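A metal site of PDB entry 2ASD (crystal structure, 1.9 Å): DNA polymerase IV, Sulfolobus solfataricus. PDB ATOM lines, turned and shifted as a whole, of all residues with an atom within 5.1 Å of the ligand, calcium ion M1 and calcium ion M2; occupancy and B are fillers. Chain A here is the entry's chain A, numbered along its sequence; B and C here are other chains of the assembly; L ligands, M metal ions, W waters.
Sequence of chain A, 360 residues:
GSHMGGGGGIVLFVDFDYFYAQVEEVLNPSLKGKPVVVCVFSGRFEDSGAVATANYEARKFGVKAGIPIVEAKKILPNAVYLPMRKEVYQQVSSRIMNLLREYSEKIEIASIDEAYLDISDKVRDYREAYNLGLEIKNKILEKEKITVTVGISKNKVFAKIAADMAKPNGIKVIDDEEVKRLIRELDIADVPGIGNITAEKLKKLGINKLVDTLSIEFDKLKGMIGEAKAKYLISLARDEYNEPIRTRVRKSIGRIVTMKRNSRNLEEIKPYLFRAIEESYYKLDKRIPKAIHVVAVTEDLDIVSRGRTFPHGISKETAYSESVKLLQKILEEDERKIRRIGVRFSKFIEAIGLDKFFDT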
ATOM      1  N   PHE A  13      28.004  32.586   6.130  1.00  0.00           N
ATOM      2  CA  PHE A  13      28.301  31.638   7.196  1.00  0.00           C
ATOM      3  C   PHE A  13      27.404  30.410   7.035  1.00  0.00           C
ATOM      4  O   PHE A  13      26.197  30.544   6.803  1.00  0.00           O
ATOM      5  CB  PHE A  13      28.068  32.308   8.542  1.00  0.00           C
ATOM      6  CG  PHE A  13      28.133  31.389   9.729  1.00  0.00           C
ATOM      7  CD1 PHE A  13      29.351  30.952  10.229  1.00  0.00           C
ATOM      8  CD2 PHE A  13      26.970  30.982  10.365  1.00  0.00           C
ATOM      9  CE1 PHE A  13      29.412  30.113  11.343  1.00  0.00           C
ATOM     10  CE2 PHE A  13      27.018  30.144  11.479  1.00  0.00           C
ATOM     11  CZ  PHE A  13      28.242  29.712  11.957  1.00  0.00           C
ATOM     12  N   ASP A  15      26.317  26.646   8.793  1.00  0.00           N
ATOM     13  CA  ASP A  15      26.231  25.905  10.037  1.00  0.00           C
ATOM     14  C   ASP A  15      25.369  24.668   9.748  1.00  0.00           C
ATOM     15  O   ASP A  15      24.189  24.818   9.440  1.00  0.00           O
ATOM     16  CB  ASP A  15      25.601  26.790  11.118  1.00  0.00           C
ATOM     17  CG  ASP A  15      25.655  26.175  12.504  1.00  0.00           C
ATOM     18  OD1 ASP A  15      25.581  24.940  12.624  1.00  0.00           O
ATOM     19  OD2 ASP A  15      25.750  26.852  13.547  1.00  0.00           O
ATOM     20  N   PHE A  16      25.945  23.480   9.823  1.00  0.00           N
ATOM     21  CA  PHE A  16      25.222  22.256   9.424  1.00  0.00           C
ATOM     22  C   PHE A  16      24.158  21.929  10.474  1.00  0.00           C
ATOM     23  O   PHE A  16      24.376  22.127  11.667  1.00  0.00           O
ATOM     24  CB  PHE A  16      26.169  21.053   9.252  1.00  0.00           C
ATOM     25  CG  PHE A  16      27.416  21.328   8.423  1.00  0.00           C
ATOM     26  CD1 PHE A  16      27.494  22.391   7.540  1.00  0.00           C
ATOM     27  CD2 PHE A  16      28.527  20.496   8.548  1.00  0.00           C
ATOM     28  CE1 PHE A  16      28.642  22.625   6.802  1.00  0.00           C
ATOM     29  CE2 PHE A  16      29.682  20.734   7.803  1.00  0.00           C
ATOM     30  CZ  PHE A  16      29.740  21.793   6.945  1.00  0.00           C
ATOM     31  N   ASP A  17      22.995  21.456  10.039  1.00  0.00           N
ATOM     32  CA  ASP A  17      21.875  21.211  10.955  1.00  0.00           C
ATOM     33  C   ASP A  17      22.046  19.909  11.728  1.00  0.00           C
ATOM     34  O   ASP A  17      22.447  18.905  11.169  1.00  0.00           O
ATOM     35  CB  ASP A  17      20.549  21.176  10.198  1.00  0.00           C
ATOM     36  CG  ASP A  17      20.230  22.464   9.472  1.00  0.00           C
ATOM     37  OD1 ASP A  17      20.492  23.566  10.016  1.00  0.00           O
ATOM     38  OD2 ASP A  17      19.701  22.480   8.334  1.00  0.00           O
ATOM     39  N   TYR A  18      21.678  19.962  13.018  1.00  0.00           N
ATOM     40  CA  TYR A  18      21.865  18.876  13.987  1.00  0.00           C
ATOM     41  C   TYR A  18      22.902  17.842  13.555  1.00  0.00           C
ATOM     42  O   TYR A  18      22.623  16.657  13.460  1.00  0.00           O
ATOM     43  CB  TYR A  18      20.524  18.230  14.353  1.00  0.00           C
ATOM     44  CG  TYR A  18      19.726  17.691  13.200  1.00  0.00           C
ATOM     45  CD1 TYR A  18      19.623  16.319  12.989  1.00  0.00           C
ATOM     46  CD2 TYR A  18      19.050  18.538  12.322  1.00  0.00           C
ATOM     47  CE1 TYR A  18      18.880  15.793  11.927  1.00  0.00           C
ATOM     48  CE2 TYR A  18      18.316  18.032  11.249  1.00  0.00           C
ATOM     49  CZ  TYR A  18      18.236  16.661  11.065  1.00  0.00           C
ATOM     50  OH  TYR A  18      17.510  16.150  10.014  1.00  0.00           O
ATOM     51  N   PHE A  19      24.127  18.310  13.362  1.00  0.00           N
ATOM     52  CA  PHE A  19      25.078  17.631  12.487  1.00  0.00           C
ATOM     53  C   PHE A  19      25.306  16.137  12.749  1.00  0.00           C
ATOM     54  O   PHE A  19      25.098  15.324  11.858  1.00  0.00           O
ATOM     55  CB  PHE A  19      26.422  18.372  12.429  1.00  0.00           C
ATOM     56  CG  PHE A  19      27.378  17.794  11.435  1.00  0.00           C
ATOM     57  CD1 PHE A  19      27.001  17.631  10.106  1.00  0.00           C
ATOM     58  CD2 PHE A  19      28.645  17.400  11.819  1.00  0.00           C
ATOM     59  CE1 PHE A  19      27.878  17.083   9.186  1.00  0.00           C
ATOM     60  CE2 PHE A  19      29.521  16.844  10.893  1.00  0.00           C
ATOM     61  CZ  PHE A  19      29.130  16.691   9.570  1.00  0.00           C
ATOM     62  N   TYR A  20      25.737  15.756  13.957  1.00  0.00           N
ATOM     63  CA  TYR A  20      26.086  14.357  14.188  1.00  0.00           C
ATOM     64  C   TYR A  20      24.883  13.435  13.991  1.00  0.00           C
ATOM     65  O   TYR A  20      25.005  12.361  13.408  1.00  0.00           O
ATOM     66  CB  TYR A  20      26.657  14.138  15.590  1.00  0.00           C
ATOM     67  CG  TYR A  20      28.006  14.772  15.877  1.00  0.00           C
ATOM     68  CD1 TYR A  20      28.635  15.595  14.946  1.00  0.00           C
ATOM     69  CD2 TYR A  20      28.650  14.524  17.084  1.00  0.00           C
ATOM     70  CE1 TYR A  20      29.878  16.167  15.218  1.00  0.00           C
ATOM     71  CE2 TYR A  20      29.865  15.090  17.369  1.00  0.00           C
ATOM     72  CZ  TYR A  20      30.479  15.915  16.439  1.00  0.00           C
ATOM     73  OH  TYR A  20      31.693  16.464  16.746  1.00  0.00           O
ATOM     74  N   VAL A  51      25.129  13.776  26.205  1.00  0.00           N
ATOM     75  CA  VAL A  51      24.599  13.880  24.849  1.00  0.00           C
ATOM     76  C   VAL A  51      25.498  14.849  24.078  1.00  0.00           C
ATOM     77  O   VAL A  51      25.765  15.957  24.547  1.00  0.00           O
ATOM     78  CB  VAL A  51      23.136  14.407  24.859  1.00  0.00           C
ATOM     79  CG1 VAL A  51      22.620  14.614  23.431  1.00  0.00           C
ATOM     80  CG2 VAL A  51      22.216  13.453  25.615  1.00  0.00           C
ATOM     81  N   ALA A  52      25.999  14.422  22.929  1.00  0.00           N
ATOM     82  CA  ALA A  52      26.721  15.318  22.036  1.00  0.00           C
ATOM     83  C   ALA A  52      25.712  16.186  21.289  1.00  0.00           C
ATOM     84  O   ALA A  52      25.871  17.404  21.193  1.00  0.00           O
ATOM     85  CB  ALA A  52      27.550  14.526  21.047  1.00  0.00           C
ATOM     86  N   THR A  53      24.678  15.551  20.745  1.00  0.00           N
ATOM     87  CA  THR A  53      23.545  16.248  20.149  1.00  0.00           C
ATOM     88  C   THR A  53      22.375  15.303  19.945  1.00  0.00           C
ATOM     89  O   THR A  53      22.515  14.088  20.034  1.00  0.00           O
ATOM     90  CB  THR A  53      23.963  16.872  18.800  1.00  0.00           C
ATOM     91  OG1 THR A  53      23.003  17.856  18.395  1.00  0.00           O
ATOM     92  CG2 THR A  53      23.943  15.844  17.675  1.00  0.00           C
ATOM     93  N   ALA A  54      21.209  15.877  19.671  1.00  0.00           N
ATOM     94  CA  ALA A  54      20.046  15.091  19.268  1.00  0.00           C
ATOM     95  C   ALA A  54      19.345  15.762  18.091  1.00  0.00           C
ATOM     96  O   ALA A  54      19.491  16.962  17.903  1.00  0.00           O
ATOM     97  CB  ALA A  54      19.096  14.926  20.451  1.00  0.00           C
ATOM     98  N   TYR A  56      15.968  17.132  15.989  1.00  0.00           N
ATOM     99  CA  TYR A  56      14.984  18.084  16.520  1.00  0.00           C
ATOM    100  C   TYR A  56      13.780  17.403  17.163  1.00  0.00           C
ATOM    101  O   TYR A  56      13.139  17.989  18.022  1.00  0.00           O
ATOM    102  CB  TYR A  56      14.558  19.107  15.445  1.00  0.00           C
ATOM    103  CG  TYR A  56      15.587  20.213  15.324  1.00  0.00           C
ATOM    104  CD1 TYR A  56      16.728  20.042  14.541  1.00  0.00           C
ATOM    105  CD2 TYR A  56      15.447  21.397  16.050  1.00  0.00           C
ATOM    106  CE1 TYR A  56      17.692  21.048  14.450  1.00  0.00           C
ATOM    107  CE2 TYR A  56      16.411  22.402  15.976  1.00  0.00           C
ATOM    108  CZ  TYR A  56      17.529  22.222  15.176  1.00  0.00           C
ATOM    109  OH  TYR A  56      18.491  23.211  15.090  1.00  0.00           O
ATOM    110  N   ARG A  59      14.918  16.787  20.559  1.00  0.00           N
ATOM    111  CA  ARG A  59      15.168  18.116  21.103  1.00  0.00           C
ATOM    112  C   ARG A  59      13.887  18.855  21.504  1.00  0.00           C
ATOM    113  O   ARG A  59      13.923  19.756  22.341  1.00  0.00           O
ATOM    114  CB  ARG A  59      15.933  18.937  20.068  1.00  0.00           C
ATOM    115  CG  ARG A  59      16.892  19.948  20.642  1.00  0.00           C
ATOM    116  CD  ARG A  59      17.623  20.724  19.572  1.00  0.00           C
ATOM    117  NE  ARG A  59      18.714  19.946  19.006  1.00  0.00           N
ATOM    118  CZ  ARG A  59      19.706  20.466  18.282  1.00  0.00           C
ATOM    119  NH1 ARG A  59      19.752  21.764  18.031  1.00  0.00           N
ATOM    120  NH2 ARG A  59      20.658  19.667  17.819  1.00  0.00           N
ATOM    121  N   ALA A  65      22.220  18.977  23.744  1.00  0.00           N
ATOM    122  CA  ALA A  65      23.651  18.804  23.971  1.00  0.00           C
ATOM    123  C   ALA A  65      24.043  19.131  25.413  1.00  0.00           C
ATOM    124  O   ALA A  65      23.547  20.099  25.987  1.00  0.00           O
ATOM    125  CB  ALA A  65      24.451  19.660  22.998  1.00  0.00           C
ATOM    126  N   GLY A  66      24.919  18.304  25.976  1.00  0.00           N
ATOM    127  CA  GLY A  66      25.504  18.561  27.275  1.00  0.00           C
ATOM    128  C   GLY A  66      24.855  17.849  28.447  1.00  0.00           C
ATOM    129  O   GLY A  66      25.493  17.693  29.484  1.00  0.00           O
ATOM    130  N   MET A  84      28.685   8.142  19.763  1.00  0.00           N
ATOM    131  CA  MET A  84      29.285   9.151  18.907  1.00  0.00           C
ATOM    132  C   MET A  84      30.384   8.497  18.090  1.00  0.00           C
ATOM    133  O   MET A  84      31.262   7.835  18.634  1.00  0.00           O
ATOM    134  CB  MET A  84      29.877  10.280  19.744  1.00  0.00           C
ATOM    135  CG  MET A  84      30.270  11.491  18.891  1.00  0.00           C
ATOM    136  SD  MET A  84      31.108  12.774  19.779  1.00  0.00           S
ATOM    137  CE  MET A  84      32.631  12.004  20.217  1.00  0.00           C
ATOM    138  N   ILE A 112      33.829  21.738  13.381  1.00  0.00           N
ATOM    139  CA  ILE A 112      33.434  20.546  12.644  1.00  0.00           C
ATOM    140  C   ILE A 112      32.232  20.769  11.721  1.00  0.00           C
ATOM    141  O   ILE A 112      32.049  20.025  10.767  1.00  0.00           O
ATOM    142  CB  ILE A 112      33.171  19.373  13.607  1.00  0.00           C
ATOM    143  CG1 ILE A 112      33.181  18.039  12.837  1.00  0.00           C
ATOM    144  CG2 ILE A 112      31.869  19.573  14.382  1.00  0.00           C
ATOM    145  CD1 ILE A 112      33.581  16.860  13.690  1.00  0.00           C
ATOM    146  N   ASP A 113      31.429  21.800  11.980  1.00  0.00           N
ATOM    147  CA  ASP A 113      30.249  22.051  11.167  1.00  0.00           C
ATOM    148  C   ASP A 113      29.979  23.522  10.807  1.00  0.00           C
ATOM    149  O   ASP A 113      28.853  23.885  10.456  1.00  0.00           O
ATOM    150  CB  ASP A 113      29.022  21.420  11.829  1.00  0.00           C
ATOM    151  CG  ASP A 113      28.462  22.264  12.969  1.00  0.00           C
ATOM    152  OD1 ASP A 113      29.196  23.037  13.633  1.00  0.00           O
ATOM    153  OD2 ASP A 113      27.273  22.179  13.262  1.00  0.00           O
ATOM    154  N   GLU A 114      31.018  24.353  10.870  1.00  0.00           N
ATOM    155  CA  GLU A 114      30.879  25.773  10.538  1.00  0.00           C
ATOM    156  C   GLU A 114      31.997  26.264   9.663  1.00  0.00           C
ATOM    157  O   GLU A 114      33.151  25.853   9.821  1.00  0.00           O
ATOM    158  CB  GLU A 114      30.923  26.628  11.790  1.00  0.00           C
ATOM    159  CG  GLU A 114      29.755  26.453  12.722  1.00  0.00           C
ATOM    160  CD  GLU A 114      30.038  27.092  14.068  1.00  0.00           C
ATOM    161  OE1 GLU A 114      31.159  26.891  14.573  1.00  0.00           O
ATOM    162  OE2 GLU A 114      29.165  27.792  14.599  1.00  0.00           O
ATOM    163  N   LYS A 160      26.824  34.917  11.829  1.00  0.00           N
ATOM    164  CA  LYS A 160      26.503  33.829  12.739  1.00  0.00           C
ATOM    165  C   LYS A 160      25.137  34.029  13.372  1.00  0.00           C
ATOM    166  O   LYS A 160      24.337  33.098  13.452  1.00  0.00           O
ATOM    167  CB  LYS A 160      27.569  33.661  13.832  1.00  0.00           C
ATOM    168  CG  LYS A 160      27.300  32.457  14.737  1.00  0.00           C
ATOM    169  CD  LYS A 160      28.328  32.317  15.850  1.00  0.00           C
ATOM    170  CE  LYS A 160      29.300  31.183  15.614  1.00  0.00           C
ATOM    171  NZ  LYS A 160      29.258  30.174  16.705  1.00  0.00           N
ATOM    172  N   LYS A 167      17.740  28.895  11.812  1.00  0.00           N
ATOM    173  CA  LYS A 167      17.960  27.449  11.978  1.00  0.00           C
ATOM    174  C   LYS A 167      16.665  26.620  11.892  1.00  0.00           C
ATOM    175  O   LYS A 167      15.566  27.166  11.880  1.00  0.00           O
ATOM    176  CB  LYS A 167      18.774  27.159  13.246  1.00  0.00           C
ATOM    177  CG  LYS A 167      20.264  27.115  12.953  1.00  0.00           C
ATOM    178  CD  LYS A 167      21.083  26.760  14.174  1.00  0.00           C
ATOM    179  CE  LYS A 167      22.541  26.973  13.877  1.00  0.00           C
ATOM    180  NZ  LYS A 167      23.399  26.668  15.057  1.00  0.00           N
ATOM    181  N   PRO A 168      16.783  25.309  12.013  1.00  0.00           N
ATOM    182  CA  PRO A 168      16.459  24.326  10.984  1.00  0.00           C
ATOM    183  C   PRO A 168      16.378  24.777   9.520  1.00  0.00           C
ATOM    184  O   PRO A 168      15.451  25.458   9.111  1.00  0.00           O
ATOM    185  CB  PRO A 168      15.142  23.777  11.519  1.00  0.00           C
ATOM    186  CG  PRO A 168      15.333  23.962  13.071  1.00  0.00           C
ATOM    187  CD  PRO A 168      16.715  24.651  13.311  1.00  0.00           C
ATOM    188  P    DA B  12      29.227  31.374  23.948  1.00  0.00           P
ATOM    189  OP1  DA B  12      28.703  32.451  23.086  1.00  0.00           O
ATOM    190  OP2  DA B  12      28.318  30.770  24.938  1.00  0.00           O
ATOM    191  O5'  DA B  12      29.787  30.210  23.019  1.00  0.00           O
ATOM    192  C5'  DA B  12      30.518  30.532  21.850  1.00  0.00           C
ATOM    193  C4'  DA B  12      30.868  29.232  21.158  1.00  0.00           C
ATOM    194  O4'  DA B  12      31.713  28.439  22.036  1.00  0.00           O
ATOM    195  C3'  DA B  12      29.624  28.392  20.827  1.00  0.00           C
ATOM    196  O3'  DA B  12      29.512  28.221  19.411  1.00  0.00           O
ATOM    197  C2'  DA B  12      29.850  27.120  21.650  1.00  0.00           C
ATOM    198  C1'  DA B  12      31.353  27.095  21.901  1.00  0.00           C
ATOM    199  N9   DA B  12      31.746  26.331  23.089  1.00  0.00           N
ATOM    200  C8   DA B  12      31.288  26.485  24.362  1.00  0.00           C
ATOM    201  N7   DA B  12      31.815  25.649  25.235  1.00  0.00           N
ATOM    202  C5   DA B  12      32.693  24.901  24.465  1.00  0.00           C
ATOM    203  C6   DA B  12      33.564  23.834  24.797  1.00  0.00           C
ATOM    204  N6   DA B  12      33.681  23.355  26.040  1.00  0.00           N
ATOM    205  N1   DA B  12      34.296  23.294  23.808  1.00  0.00           N
ATOM    206  C2   DA B  12      34.180  23.789  22.560  1.00  0.00           C
ATOM    207  N3   DA B  12      33.383  24.785  22.125  1.00  0.00           N
ATOM    208  C4   DA B  12      32.664  25.298  23.148  1.00  0.00           C
ATOM    209  P   DDG B  13      28.400  27.275  18.776  1.00  0.00           P
ATOM    210  OP1 DDG B  13      27.971  27.872  17.481  1.00  0.00           O
ATOM    211  OP2 DDG B  13      27.364  26.910  19.755  1.00  0.00           O
ATOM    212  O5' DDG B  13      29.258  25.952  18.477  1.00  0.00           O
ATOM    213  C5' DDG B  13      30.464  26.057  17.733  1.00  0.00           C
ATOM    214  C4' DDG B  13      31.158  24.714  17.626  1.00  0.00           C
ATOM    215  O4' DDG B  13      31.672  24.326  18.928  1.00  0.00           O
ATOM    216  C3' DDG B  13      30.295  23.573  17.108  1.00  0.00           C
ATOM    217  C2' DDG B  13      30.392  22.472  18.161  1.00  0.00           C
ATOM    218  C1' DDG B  13      31.520  22.930  19.094  1.00  0.00           C
ATOM    219  N9  DDG B  13      31.235  22.689  20.494  1.00  0.00           N
ATOM    220  C8  DDG B  13      30.401  23.432  21.314  1.00  0.00           C
ATOM    221  N7  DDG B  13      30.350  22.987  22.541  1.00  0.00           N
ATOM    222  C5  DDG B  13      31.209  21.892  22.526  1.00  0.00           C
ATOM    223  C6  DDG B  13      31.568  21.004  23.568  1.00  0.00           C
ATOM    224  O6  DDG B  13      31.177  21.029  24.730  1.00  0.00           O
ATOM    225  N1  DDG B  13      32.453  20.009  23.161  1.00  0.00           N
ATOM    226  C2  DDG B  13      32.954  19.921  21.893  1.00  0.00           C
ATOM    227  N2  DDG B  13      33.803  18.910  21.666  1.00  0.00           N
ATOM    228  N3  DDG B  13      32.625  20.744  20.883  1.00  0.00           N
ATOM    229  C4  DDG B  13      31.757  21.700  21.288  1.00  0.00           C
ATOM    230  P   8OG C   6      30.539  11.039  32.500  1.00  0.00           P
ATOM    231  OP1 8OG C   6      30.444   9.621  33.021  1.00  0.00           O
ATOM    232  OP2 8OG C   6      31.444  12.038  33.151  1.00  0.00           O
ATOM    233  O5' 8OG C   6      30.915  10.978  30.949  1.00  0.00           O
ATOM    234  C5' 8OG C   6      30.818  12.158  30.176  1.00  0.00           C
ATOM    235  C4' 8OG C   6      31.560  12.088  28.875  1.00  0.00           C
ATOM    236  O4' 8OG C   6      30.957  12.768  27.769  1.00  0.00           O
ATOM    237  C3' 8OG C   6      32.873  12.128  28.719  1.00  0.00           C
ATOM    238  O3' 8OG C   6      33.377  11.197  28.094  1.00  0.00           O
ATOM    239  C2' 8OG C   6      33.204  13.552  28.367  1.00  0.00           C
ATOM    240  C1' 8OG C   6      31.896  13.878  27.711  1.00  0.00           C
ATOM    241  N9  8OG C   6      31.293  15.067  27.503  1.00  0.00           N
ATOM    242  C8  8OG C   6      30.722  15.726  28.488  1.00  0.00           C
ATOM    243  N7  8OG C   6      30.061  16.807  28.049  1.00  0.00           N
ATOM    244  C5  8OG C   6      30.173  16.773  26.714  1.00  0.00           C
ATOM    245  C6  8OG C   6      29.712  17.603  25.600  1.00  0.00           C
ATOM    246  O6  8OG C   6      29.028  18.626  25.831  1.00  0.00           O
ATOM    247  N1  8OG C   6      30.036  17.233  24.356  1.00  0.00           N
ATOM    248  C2  8OG C   6      30.775  16.135  24.080  1.00  0.00           C
ATOM    249  N2  8OG C   6      31.048  15.837  22.782  1.00  0.00           N
ATOM    250  N3  8OG C   6      31.232  15.325  25.050  1.00  0.00           N
ATOM    251  C4  8OG C   6      30.968  15.573  26.329  1.00  0.00           C
ATOM    252  O8  8OG C   6      30.848  15.407  29.717  1.00  0.00           O
HETATM  253  N1  LIG L   1      28.729  19.044  19.826  1.00  0.00           N
HETATM  254  C1  LIG L   1      29.215  18.344  20.878  1.00  0.00           C
HETATM  255  N2  LIG L   1      29.003  18.773  22.125  1.00  0.00           N
HETATM  256  C2  LIG L   1      28.292  19.885  22.359  1.00  0.00           C
HETATM  257  C3  LIG L   1      27.767  20.613  21.309  1.00  0.00           C
HETATM  258  C4  LIG L   1      28.003  20.159  20.027  1.00  0.00           C
HETATM  259  O1  LIG L   1      29.870  17.289  20.711  1.00  0.00           O
HETATM  260  N3  LIG L   1      28.082  20.304  23.669  1.00  0.00           N
HETATM  261  C5  LIG L   1      28.959  18.559  18.467  1.00  0.00           C
HETATM  262  C6  LIG L   1      27.709  17.791  18.022  1.00  0.00           C
HETATM  263  C7  LIG L   1      26.954  18.772  17.146  1.00  0.00           C
HETATM  264  C8  LIG L   1      28.087  19.584  16.527  1.00  0.00           C
HETATM  265  O2  LIG L   1      29.084  19.621  17.542  1.00  0.00           O
HETATM  266  O3  LIG L   1      26.147  18.119  16.181  1.00  0.00           O
HETATM  267  C9  LIG L   1      27.692  20.979  16.090  1.00  0.00           C
HETATM  268  O4  LIG L   1      27.207  21.725  17.196  1.00  0.00           O
HETATM  269  P1  LIG L   1      25.881  22.450  17.135  1.00  0.00           P
HETATM  270  O5  LIG L   1      25.803  23.313  18.347  1.00  0.00           O
HETATM  271  O6  LIG L   1      25.852  23.265  15.863  1.00  0.00           O
HETATM  272  O7  LIG L   1      24.751  21.469  17.240  1.00  0.00           O
HETATM  273  P2  LIG L   1      23.868  20.905  16.154  1.00  0.00           P
HETATM  274  O8  LIG L   1      24.420  21.032  14.775  1.00  0.00           O
HETATM  275  O9  LIG L   1      23.674  19.444  16.465  1.00  0.00           O
HETATM  276  O10 LIG L   1      22.536  21.627  16.250  1.00  0.00           O
HETATM  277  P3  LIG L   1      22.097  22.878  15.476  1.00  0.00           P
HETATM  278  O11 LIG L   1      23.110  23.556  14.571  1.00  0.00           O
HETATM  279  O12 LIG L   1      21.708  23.920  16.504  1.00  0.00           O
HETATM  280  O13 LIG L   1      20.956  22.491  14.568  1.00  0.00           O
HETATM  281 CA    CA M   1      25.133  22.934  13.678  1.00  0.00          CA
HETATM  282 CA    CA M   2      27.179  27.003  15.476  1.00  0.00          CA
HETATM  283  O   HOH W   1      27.854  24.775  15.161  1.00  0.00           O
HETATM  284  O   HOH W   2      27.034  24.435  20.675  1.00  0.00           O
HETATM  285  O   HOH W   3      26.288  22.631  24.337  1.00  0.00           O
HETATM  286  O   HOH W   4      25.709  28.973  15.623  1.00  0.00           O
HETATM  287  O   HOH W   5      32.071  16.642  19.399  1.00  0.00           O
HETATM  288  O   HOH W   6      25.482  26.112  16.655  1.00  0.00           O
HETATM  289  O   HOH W   7      18.932  25.210  16.939  1.00  0.00           O
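A nitrogen (N3) of the ligand is in hydrogen-bond range of O6 of 8OG 6 of chain C.
N of Phe 19 sits at hydrogen-bond distance from O9 of the ligand, 3.3 Å away.
O13 of the ligand sits at hydrogen-bond distance from N of Tyr 18, at 3.1 Å.
N of Tyr 20 is in hydrogen-bond range of O3 of the ligand, at 3.3 Å.
O9 of the ligand sits at hydrogen-bond distance from OG1 of Thr 53, at 2.6 Å.
The guanidinium group (NH1) of Arg 59 is in salt-bridge range of an oxygen (O12) of the ligand, 3.3 Å away.
An oxygen (O12) of the ligand lies within salt-bridge range of the side-chain amino group (NZ) of Lys 167, at 3.5 Å.
OH of Tyr 56 is in hydrogen-bond range of O13 of the ligand (2.6 Å).
N3 of the ligand sits at hydrogen-bond distance from O6 of DDG 13 of chain B (3.4 Å).
Merely in contact with calcium ion M2: Lys 167 (3.8 Å) and Lys 160 (3.99 Å).
Of the 25 residues printed, 5 come within 4 Å of calcium ion M2.
The backbone carbonyl oxygen (O) of Phe 16 binds calcium ion M1 (2.3 Å).
Calcium ion M1 is bound by O11 of the ligand (2.3 Å).
Calcium ion M1 is bound by the side-chain carboxylate (OD2) of Asp 113 (2.3 Å).
O8 of the ligand is bound to calcium ion M1, at 2.3 Å.
Calcium ion M1 is bound by OD1 of Asp 15.
Calcium ion M1 is bound by O6 of the ligand (2.3 Å).
Water W6 bridges NZ of Lys 167 (2.7 Å) and O5 of the ligand (3.3 Å).
Water W5 lies within hydrogen-bond range of O1 of the ligand (2.6 Å) and OH of Tyr 20 (2.7 Å).
Water W2 lies within hydrogen-bond range of OP2 of DDG 13 of chain B and O5 of the ligand.
Water W7 lies within hydrogen-bond range of OH of Tyr 56 and O12 of the ligand.
Calcium ion M2 is bound by water W6 (2.3 Å), the side-chain carboxylate of Glu 114 (2.3 Å), OP1 of DDG 13 of chain B (2.3 Å), water W1 (2.3 Å), the side-chain carboxylate of Asp 15 (2.4 Å) and water W4 (2.5 Å).
Residues that only touch the ligand: Asp 17, Ala 52 and Ala 65.
Of the 25 residues printed, 15 come within 4 Å of the ligand.
The side-chain amino group (NZ) of Lys 167 lies close to the side-chain carboxylate (OD2) of Asp 15, at 2.8 Å.
The side-chain hydroxyl (OG1) of Thr 53 sits at hydrogen-bond distance from the guanidinium group (NH2) of Arg 59, at 3.0 Å.
OE2 of Glu 114 sits close to NZ of Lys 160 (3.2 Å).
O3' of DA 12 of chain B sits at hydrogen-bond distance from the side-chain amino group of Lys 160 (3.3 Å).
The side-chain amino group (NZ) of Lys 160 sits close to OP1 of DDG 13 of chain B (2.7 Å).
The backbone carbonyl oxygen (O) of Ala 54 sits at hydrogen-bond distance from the guanidinium group (NH2) of Arg 59 (2.9 Å).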
